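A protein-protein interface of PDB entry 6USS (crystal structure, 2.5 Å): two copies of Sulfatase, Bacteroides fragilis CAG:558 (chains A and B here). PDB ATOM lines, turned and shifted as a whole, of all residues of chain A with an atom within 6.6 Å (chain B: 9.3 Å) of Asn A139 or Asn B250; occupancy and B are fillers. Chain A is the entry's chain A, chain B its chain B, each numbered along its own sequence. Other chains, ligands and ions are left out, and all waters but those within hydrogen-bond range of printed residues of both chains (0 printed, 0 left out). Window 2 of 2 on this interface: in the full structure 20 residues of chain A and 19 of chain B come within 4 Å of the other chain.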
ATOM      1  N   LYS A 113     -14.118 -30.757  -0.461  1.00  0.00           N
ATOM      2  CA  LYS A 113     -14.253 -31.299   0.889  1.00  0.00           C
ATOM      3  C   LYS A 113     -15.533 -32.121   1.024  1.00  0.00           C
ATOM      4  O   LYS A 113     -16.631 -31.648   0.700  1.00  0.00           O
ATOM      5  CB  LYS A 113     -14.238 -30.183   1.921  1.00  0.00           C
ATOM      6  CG  LYS A 113     -14.431 -30.660   3.362  1.00  0.00           C
ATOM      7  CD  LYS A 113     -14.198 -29.492   4.363  1.00  0.00           C
ATOM      8  CE  LYS A 113     -14.311 -29.953   5.802  1.00  0.00           C
ATOM      9  NZ  LYS A 113     -13.704 -28.976   6.727  1.00  0.00           N
ATOM     10  N   VAL A 137      -3.566 -35.304  12.022  1.00  0.00           N
ATOM     11  CA  VAL A 137      -4.401 -35.169  13.215  1.00  0.00           C
ATOM     12  C   VAL A 137      -5.545 -36.169  13.135  1.00  0.00           C
ATOM     13  O   VAL A 137      -5.867 -36.656  12.041  1.00  0.00           O
ATOM     14  CB  VAL A 137      -4.918 -33.735  13.364  1.00  0.00           C
ATOM     15  CG1 VAL A 137      -3.775 -32.836  13.739  1.00  0.00           C
ATOM     16  CG2 VAL A 137      -5.538 -33.278  12.067  1.00  0.00           C
ATOM     17  N   PRO A 138      -6.156 -36.533  14.247  1.00  0.00           N
ATOM     18  CA  PRO A 138      -7.269 -37.492  14.192  1.00  0.00           C
ATOM     19  C   PRO A 138      -8.621 -36.794  14.078  1.00  0.00           C
ATOM     20  O   PRO A 138      -8.690 -35.557  14.091  1.00  0.00           O
ATOM     21  CB  PRO A 138      -7.125 -38.259  15.511  1.00  0.00           C
ATOM     22  CG  PRO A 138      -6.549 -37.223  16.455  1.00  0.00           C
ATOM     23  CD  PRO A 138      -5.656 -36.329  15.620  1.00  0.00           C
ATOM     24  N   ASN A 139      -9.694 -37.585  13.938  1.00  0.00           N
ATOM     25  CA  ASN A 139     -11.076 -37.091  13.952  1.00  0.00           C
ATOM     26  C   ASN A 139     -11.357 -36.117  12.811  1.00  0.00           C
ATOM     27  O   ASN A 139     -12.201 -35.224  12.936  1.00  0.00           O
ATOM     28  CB  ASN A 139     -11.426 -36.435  15.293  1.00  0.00           C
ATOM     29  CG  ASN A 139     -11.149 -37.349  16.488  1.00  0.00           C
ATOM     30  OD1 ASN A 139     -11.493 -38.532  16.477  1.00  0.00           O
ATOM     31  ND2 ASN A 139     -10.521 -36.798  17.522  1.00  0.00           N
ATOM     32  N   ILE A 140     -10.662 -36.259  11.690  1.00  0.00           N
ATOM     33  CA  ILE A 140     -10.960 -35.472  10.499  1.00  0.00           C
ATOM     34  C   ILE A 140     -11.716 -36.357   9.516  1.00  0.00           C
ATOM     35  O   ILE A 140     -11.162 -37.333   8.993  1.00  0.00           O
ATOM     36  CB  ILE A 140      -9.691 -34.888   9.868  1.00  0.00           C
ATOM     37  CG1 ILE A 140      -8.959 -34.030  10.898  1.00  0.00           C
ATOM     38  CG2 ILE A 140     -10.080 -34.020   8.709  1.00  0.00           C
ATOM     39  CD1 ILE A 140      -9.800 -32.908  11.467  1.00  0.00           C
ATOM     40  N   ASP A 141     -12.963 -35.960   9.235  1.00  0.00           N
ATOM     41  CA  ASP A 141     -14.043 -36.768   8.665  1.00  0.00           C
ATOM     42  C   ASP A 141     -13.593 -37.904   7.754  1.00  0.00           C
ATOM     43  O   ASP A 141     -13.684 -39.075   8.147  1.00  0.00           O
ATOM     44  CB  ASP A 141     -15.038 -35.877   7.904  1.00  0.00           C
ATOM     45  CG  ASP A 141     -16.083 -36.688   7.145  1.00  0.00           C
ATOM     46  OD1 ASP A 141     -16.598 -37.667   7.738  1.00  0.00           O
ATOM     47  OD2 ASP A 141     -16.386 -36.362   5.965  1.00  0.00           O
ATOM     48  N   THR A 143     -10.538 -38.861   6.269  1.00  0.00           N
ATOM     49  CA  THR A 143      -9.098 -38.817   6.086  1.00  0.00           C
ATOM     50  C   THR A 143      -8.454 -40.071   6.651  1.00  0.00           C
ATOM     51  O   THR A 143      -9.011 -40.733   7.532  1.00  0.00           O
ATOM     52  CB  THR A 143      -8.478 -37.588   6.774  1.00  0.00           C
ATOM     53  OG1 THR A 143      -8.647 -37.699   8.196  1.00  0.00           O
ATOM     54  CG2 THR A 143      -9.127 -36.306   6.259  1.00  0.00           C
ATOM     55  N   GLN A 145      -5.354 -40.793   8.897  1.00  0.00           N
ATOM     56  CA  GLN A 145      -4.398 -40.143   9.787  1.00  0.00           C
ATOM     57  C   GLN A 145      -3.056 -40.848   9.671  1.00  0.00           C
ATOM     58  O   GLN A 145      -2.994 -42.082   9.680  1.00  0.00           O
ATOM     59  CB  GLN A 145      -4.869 -40.172  11.240  1.00  0.00           C
ATOM     60  CG  GLN A 145      -3.817 -39.619  12.222  1.00  0.00           C
ATOM     61  CD  GLN A 145      -4.256 -39.645  13.691  1.00  0.00           C
ATOM     62  OE1 GLN A 145      -5.314 -40.184  14.026  1.00  0.00           O
ATOM     63  NE2 GLN A 145      -3.438 -39.060  14.567  1.00  0.00           N
ATOM     64  N   PRO A 174      -7.149 -30.272   7.098  1.00  0.00           N
ATOM     65  CA  PRO A 174      -5.778 -29.941   7.552  1.00  0.00           C
ATOM     66  C   PRO A 174      -4.672 -30.277   6.559  1.00  0.00           C
ATOM     67  O   PRO A 174      -3.706 -29.513   6.442  1.00  0.00           O
ATOM     68  CB  PRO A 174      -5.632 -30.753   8.847  1.00  0.00           C
ATOM     69  CG  PRO A 174      -7.033 -30.852   9.376  1.00  0.00           C
ATOM     70  CD  PRO A 174      -7.929 -30.960   8.151  1.00  0.00           C
ATOM     71  N   ARG B  33     -11.478 -29.798  24.740  1.00  0.00           N
ATOM     72  CA  ARG B  33     -10.203 -29.061  24.778  1.00  0.00           C
ATOM     73  C   ARG B  33     -10.347 -27.647  24.229  1.00  0.00           C
ATOM     74  O   ARG B  33     -10.756 -27.437  23.090  1.00  0.00           O
ATOM     75  CB  ARG B  33      -9.109 -29.790  24.003  1.00  0.00           C
ATOM     76  CG  ARG B  33      -8.493 -30.964  24.764  1.00  0.00           C
ATOM     77  CD  ARG B  33      -7.217 -31.525  24.114  1.00  0.00           C
ATOM     78  NE  ARG B  33      -7.350 -31.659  22.670  1.00  0.00           N
ATOM     79  CZ  ARG B  33      -6.346 -31.983  21.858  1.00  0.00           C
ATOM     80  NH1 ARG B  33      -5.122 -32.225  22.338  1.00  0.00           N
ATOM     81  NH2 ARG B  33      -6.562 -32.076  20.561  1.00  0.00           N
ATOM     82  N   ASN B  35      -9.776 -23.867  22.772  1.00  0.00           N
ATOM     83  CA  ASN B  35      -8.894 -23.020  21.995  1.00  0.00           C
ATOM     84  C   ASN B  35      -8.131 -22.103  22.939  1.00  0.00           C
ATOM     85  O   ASN B  35      -8.579 -21.814  24.051  1.00  0.00           O
ATOM     86  CB  ASN B  35      -9.694 -22.190  20.995  1.00  0.00           C
ATOM     87  CG  ASN B  35     -10.642 -23.029  20.180  1.00  0.00           C
ATOM     88  OD1 ASN B  35     -10.214 -23.952  19.506  1.00  0.00           O
ATOM     89  ND2 ASN B  35     -11.935 -22.706  20.220  1.00  0.00           N
ATOM     90  N   ASN B 156       0.407 -32.214  19.483  1.00  0.00           N
ATOM     91  CA  ASN B 156      -0.694 -32.769  20.263  1.00  0.00           C
ATOM     92  C   ASN B 156      -2.062 -32.500  19.627  1.00  0.00           C
ATOM     93  O   ASN B 156      -3.093 -32.772  20.256  1.00  0.00           O
ATOM     94  CB  ASN B 156      -0.645 -32.245  21.704  1.00  0.00           C
ATOM     95  CG  ASN B 156       0.379 -32.986  22.564  1.00  0.00           C
ATOM     96  OD1 ASN B 156       0.023 -33.904  23.300  1.00  0.00           O
ATOM     97  ND2 ASN B 156       1.655 -32.587  22.476  1.00  0.00           N
ATOM     98  N   GLY B 157      -2.091 -31.983  18.398  1.00  0.00           N
ATOM     99  CA  GLY B 157      -3.316 -31.838  17.645  1.00  0.00           C
ATOM    100  C   GLY B 157      -3.899 -30.438  17.563  1.00  0.00           C
ATOM    101  O   GLY B 157      -4.972 -30.269  16.961  1.00  0.00           O
ATOM    102  N   TYR B 158      -3.239 -29.435  18.135  1.00  0.00           N
ATOM    103  CA  TYR B 158      -3.687 -28.057  17.974  1.00  0.00           C
ATOM    104  C   TYR B 158      -3.286 -27.521  16.602  1.00  0.00           C
ATOM    105  O   TYR B 158      -2.189 -27.798  16.112  1.00  0.00           O
ATOM    106  CB  TYR B 158      -3.099 -27.167  19.074  1.00  0.00           C
ATOM    107  CG  TYR B 158      -3.918 -27.139  20.341  1.00  0.00           C
ATOM    108  CD1 TYR B 158      -3.932 -28.229  21.208  1.00  0.00           C
ATOM    109  CD2 TYR B 158      -4.694 -26.029  20.667  1.00  0.00           C
ATOM    110  CE1 TYR B 158      -4.696 -28.217  22.369  1.00  0.00           C
ATOM    111  CE2 TYR B 158      -5.447 -26.002  21.822  1.00  0.00           C
ATOM    112  CZ  TYR B 158      -5.445 -27.096  22.671  1.00  0.00           C
ATOM    113  OH  TYR B 158      -6.202 -27.053  23.829  1.00  0.00           O
ATOM    114  N   HIS B 159      -4.194 -26.764  15.983  1.00  0.00           N
ATOM    115  CA  HIS B 159      -3.877 -25.933  14.825  1.00  0.00           C
ATOM    116  C   HIS B 159      -3.257 -24.621  15.318  1.00  0.00           C
ATOM    117  O   HIS B 159      -3.893 -23.880  16.077  1.00  0.00           O
ATOM    118  CB  HIS B 159      -5.146 -25.672  14.009  1.00  0.00           C
ATOM    119  CG  HIS B 159      -4.962 -24.714  12.868  1.00  0.00           C
ATOM    120  ND1 HIS B 159      -4.248 -25.030  11.732  1.00  0.00           N
ATOM    121  CD2 HIS B 159      -5.415 -23.452  12.682  1.00  0.00           C
ATOM    122  CE1 HIS B 159      -4.263 -24.002  10.901  1.00  0.00           C
ATOM    123  NE2 HIS B 159      -4.963 -23.032  11.454  1.00  0.00           N
ATOM    124  N   HIS B 245     -10.666 -19.692   8.831  1.00  0.00           N
ATOM    125  CA  HIS B 245     -10.112 -20.905   8.245  1.00  0.00           C
ATOM    126  C   HIS B 245      -9.991 -22.021   9.279  1.00  0.00           C
ATOM    127  O   HIS B 245     -10.269 -23.185   8.963  1.00  0.00           O
ATOM    128  CB  HIS B 245      -8.761 -20.630   7.601  1.00  0.00           C
ATOM    129  CG  HIS B 245      -8.446 -21.581   6.502  1.00  0.00           C
ATOM    130  ND1 HIS B 245      -7.840 -21.194   5.327  1.00  0.00           N
ATOM    131  CD2 HIS B 245      -8.699 -22.905   6.377  1.00  0.00           C
ATOM    132  CE1 HIS B 245      -7.714 -22.244   4.534  1.00  0.00           C
ATOM    133  NE2 HIS B 245      -8.223 -23.297   5.151  1.00  0.00           N
ATOM    134  N   ALA B 246      -9.587 -21.699  10.516  1.00  0.00           N
ATOM    135  CA  ALA B 246      -9.446 -22.753  11.523  1.00  0.00           C
ATOM    136  C   ALA B 246     -10.773 -23.465  11.792  1.00  0.00           C
ATOM    137  O   ALA B 246     -10.780 -24.661  12.099  1.00  0.00           O
ATOM    138  CB  ALA B 246      -8.871 -22.186  12.828  1.00  0.00           C
ATOM    139  N   LYS B 247     -11.902 -22.758  11.661  1.00  0.00           N
ATOM    140  CA  LYS B 247     -13.206 -23.364  11.904  1.00  0.00           C
ATOM    141  C   LYS B 247     -13.543 -24.472  10.911  1.00  0.00           C
ATOM    142  O   LYS B 247     -14.453 -25.257  11.185  1.00  0.00           O
ATOM    143  CB  LYS B 247     -14.294 -22.286  11.898  1.00  0.00           C
ATOM    144  CG  LYS B 247     -14.582 -21.771  13.301  1.00  0.00           C
ATOM    145  CD  LYS B 247     -15.729 -20.766  13.378  1.00  0.00           C
ATOM    146  CE  LYS B 247     -16.864 -21.078  12.413  1.00  0.00           C
ATOM    147  NZ  LYS B 247     -18.081 -20.271  12.717  1.00  0.00           N
ATOM    148  N   GLU B 248     -12.824 -24.574   9.786  1.00  0.00           N
ATOM    149  CA  GLU B 248     -12.957 -25.691   8.850  1.00  0.00           C
ATOM    150  C   GLU B 248     -12.285 -26.974   9.338  1.00  0.00           C
ATOM    151  O   GLU B 248     -12.535 -28.052   8.770  1.00  0.00           O
ATOM    152  CB  GLU B 248     -12.366 -25.309   7.491  1.00  0.00           C
ATOM    153  CG  GLU B 248     -13.121 -24.200   6.765  1.00  0.00           C
ATOM    154  CD  GLU B 248     -14.469 -24.669   6.231  1.00  0.00           C
ATOM    155  OE1 GLU B 248     -14.627 -25.889   5.937  1.00  0.00           O
ATOM    156  OE2 GLU B 248     -15.374 -23.808   6.125  1.00  0.00           O
ATOM    157  N   TYR B 249     -11.452 -26.891  10.372  1.00  0.00           N
ATOM    158  CA  TYR B 249     -10.676 -28.023  10.865  1.00  0.00           C
ATOM    159  C   TYR B 249     -11.236 -28.488  12.202  1.00  0.00           C
ATOM    160  O   TYR B 249     -11.463 -27.670  13.097  1.00  0.00           O
ATOM    161  CB  TYR B 249      -9.201 -27.646  11.040  1.00  0.00           C
ATOM    162  CG  TYR B 249      -8.507 -27.136   9.797  1.00  0.00           C
ATOM    163  CD1 TYR B 249      -9.030 -27.359   8.523  1.00  0.00           C
ATOM    164  CD2 TYR B 249      -7.309 -26.462   9.902  1.00  0.00           C
ATOM    165  CE1 TYR B 249      -8.370 -26.895   7.395  1.00  0.00           C
ATOM    166  CE2 TYR B 249      -6.640 -26.012   8.791  1.00  0.00           C
ATOM    167  CZ  TYR B 249      -7.164 -26.220   7.542  1.00  0.00           C
ATOM    168  OH  TYR B 249      -6.469 -25.737   6.448  1.00  0.00           O
ATOM    169  N   ASN B 250     -11.417 -29.804  12.349  1.00  0.00           N
ATOM    170  CA  ASN B 250     -11.957 -30.384  13.583  1.00  0.00           C
ATOM    171  C   ASN B 250     -10.832 -30.612  14.599  1.00  0.00           C
ATOM    172  O   ASN B 250     -10.500 -31.734  14.986  1.00  0.00           O
ATOM    173  CB  ASN B 250     -12.704 -31.674  13.277  1.00  0.00           C
ATOM    174  CG  ASN B 250     -13.448 -32.211  14.483  1.00  0.00           C
ATOM    175  OD1 ASN B 250     -13.880 -31.447  15.347  1.00  0.00           O
ATOM    176  ND2 ASN B 250     -13.578 -33.531  14.559  1.00  0.00           N
ATOM    177  N   GLN B 251     -10.236 -29.498  15.026  1.00  0.00           N
ATOM    178  CA  GLN B 251      -9.164 -29.480  16.016  1.00  0.00           C
ATOM    179  C   GLN B 251      -9.187 -28.120  16.696  1.00  0.00           C
ATOM    180  O   GLN B 251      -9.588 -27.137  16.069  1.00  0.00           O
ATOM    181  CB  GLN B 251      -7.790 -29.736  15.370  1.00  0.00           C
ATOM    182  CG  GLN B 251      -7.537 -29.017  14.040  1.00  0.00           C
ATOM    183  CD  GLN B 251      -6.127 -29.271  13.482  1.00  0.00           C
ATOM    184  OE1 GLN B 251      -5.255 -29.816  14.167  1.00  0.00           O
ATOM    185  NE2 GLN B 251      -5.912 -28.891  12.232  1.00  0.00           N
ATOM    186  N   PRO B 252      -8.793 -28.031  17.967  1.00  0.00           N
ATOM    187  CA  PRO B 252      -8.720 -26.722  18.622  1.00  0.00           C
ATOM    188  C   PRO B 252      -7.578 -25.897  18.044  1.00  0.00           C
ATOM    189  O   PRO B 252      -6.625 -26.425  17.465  1.00  0.00           O
ATOM    190  CB  PRO B 252      -8.456 -27.082  20.086  1.00  0.00           C
ATOM    191  CG  PRO B 252      -7.713 -28.356  20.004  1.00  0.00           C
ATOM    192  CD  PRO B 252      -8.241 -29.097  18.824  1.00  0.00           C
ATOM    193  N   PHE B 253      -7.678 -24.584  18.196  1.00  0.00           N
ATOM    194  CA  PHE B 253      -6.612 -23.726  17.710  1.00  0.00           C
ATOM    195  C   PHE B 253      -5.863 -23.049  18.854  1.00  0.00           C
ATOM    196  O   PHE B 253      -6.381 -22.852  19.961  1.00  0.00           O
ATOM    197  CB  PHE B 253      -7.141 -22.674  16.726  1.00  0.00           C
ATOM    198  CG  PHE B 253      -8.103 -21.685  17.326  1.00  0.00           C
ATOM    199  CD1 PHE B 253      -7.646 -20.574  18.036  1.00  0.00           C
ATOM    200  CD2 PHE B 253      -9.465 -21.840  17.152  1.00  0.00           C
ATOM    201  CE1 PHE B 253      -8.533 -19.651  18.577  1.00  0.00           C
ATOM    202  CE2 PHE B 253     -10.365 -20.921  17.695  1.00  0.00           C
ATOM    203  CZ  PHE B 253      -9.896 -19.828  18.399  1.00  0.00           C
ATOM    204  N   GLU B 311     -17.541 -19.484  19.821  1.00  0.00           N
ATOM    205  CA  GLU B 311     -16.315 -20.049  20.358  1.00  0.00           C
ATOM    206  C   GLU B 311     -15.961 -19.497  21.726  1.00  0.00           C
ATOM    207  O   GLU B 311     -14.996 -19.973  22.334  1.00  0.00           O
ATOM    208  CB  GLU B 311     -15.161 -19.806  19.385  1.00  0.00           C
ATOM    209  CG  GLU B 311     -15.413 -20.382  18.003  1.00  0.00           C
ATOM    210  CD  GLU B 311     -14.934 -21.814  17.882  1.00  0.00           C
ATOM    211  OE1 GLU B 311     -14.697 -22.268  16.739  1.00  0.00           O
ATOM    212  OE2 GLU B 311     -14.790 -22.489  18.931  1.00  0.00           O
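The side-chain amino group of Lys A113 lies within salt-bridge range of the side-chain carboxylate of Glu B248 (3.3 Å).
The side-chain amide nitrogen of Asn B250 lies within hydrogen-bond range of the backbone carbonyl oxygen of Asn A139, at 2.7 Å.
The side-chain hydroxyl of Thr A143 is in hydrogen-bond range of the backbone carbonyl oxygen of Ile A140, 2.7 Å away.
The backbone carbonyl oxygen (O) of Gly B157 lies close to the side-chain amide oxygen (OE1) of Gln B251.
The side-chain hydroxyl of Tyr B249 is in hydrogen-bond range of a ring nitrogen (NE2) of His B245, 3.3 Å away.
CG1 of Val A137 touches OE1 of Gln B251, 3.4 Å away.
Ile A140 touches Asn B250 (CD1 to N, 3.6 Å).
Tyr B249 touches Pro A174 (CE1 to N, 3.6 Å).
Pro A174 touches Gln B251 (CG to NE2, 3.6 Å).
Printed residues of chain B within 4 Å of Val A137: Gln B251.
No residue of chain B comes within 4 Å of Pro A138.
Asn A139 touches just one residue of chain B: Asn B250.
Of the printed residues of chain A, Tyr B249 touches Pro A174 (3.6 Å).
Asn B250 touches just these residues of chain A: Asn A139 (2.7 Å) and Ile A140 (3.6 Å).
The nearest residue of chain B that does not touch Asn A139 is Gln B251 (6.4 Å).
Of the 9 printed residues of chain A, 5 touch a printed residue of chain B.
Hydrophobic or aromatic side chains of chain A within 4 Å of the printed part of chain B: Val A137, Ile A140 and Pro A174.
Along chain A the printed residues that touch a printed residue of chain B span positions 113 to 174.
Printed residues of chain B that touch a printed residue of chain A: Glu B248, Tyr B249, Asn B250 and Gln B251.
Hydrophobic or aromatic side chains of chain B within 4 Å of the printed part of chain A: Tyr B249.
No position is printed for both chains.
Of the 6 pairs that touch across the chains among the printed residues, none has its exchanged pair printed and touching as well.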
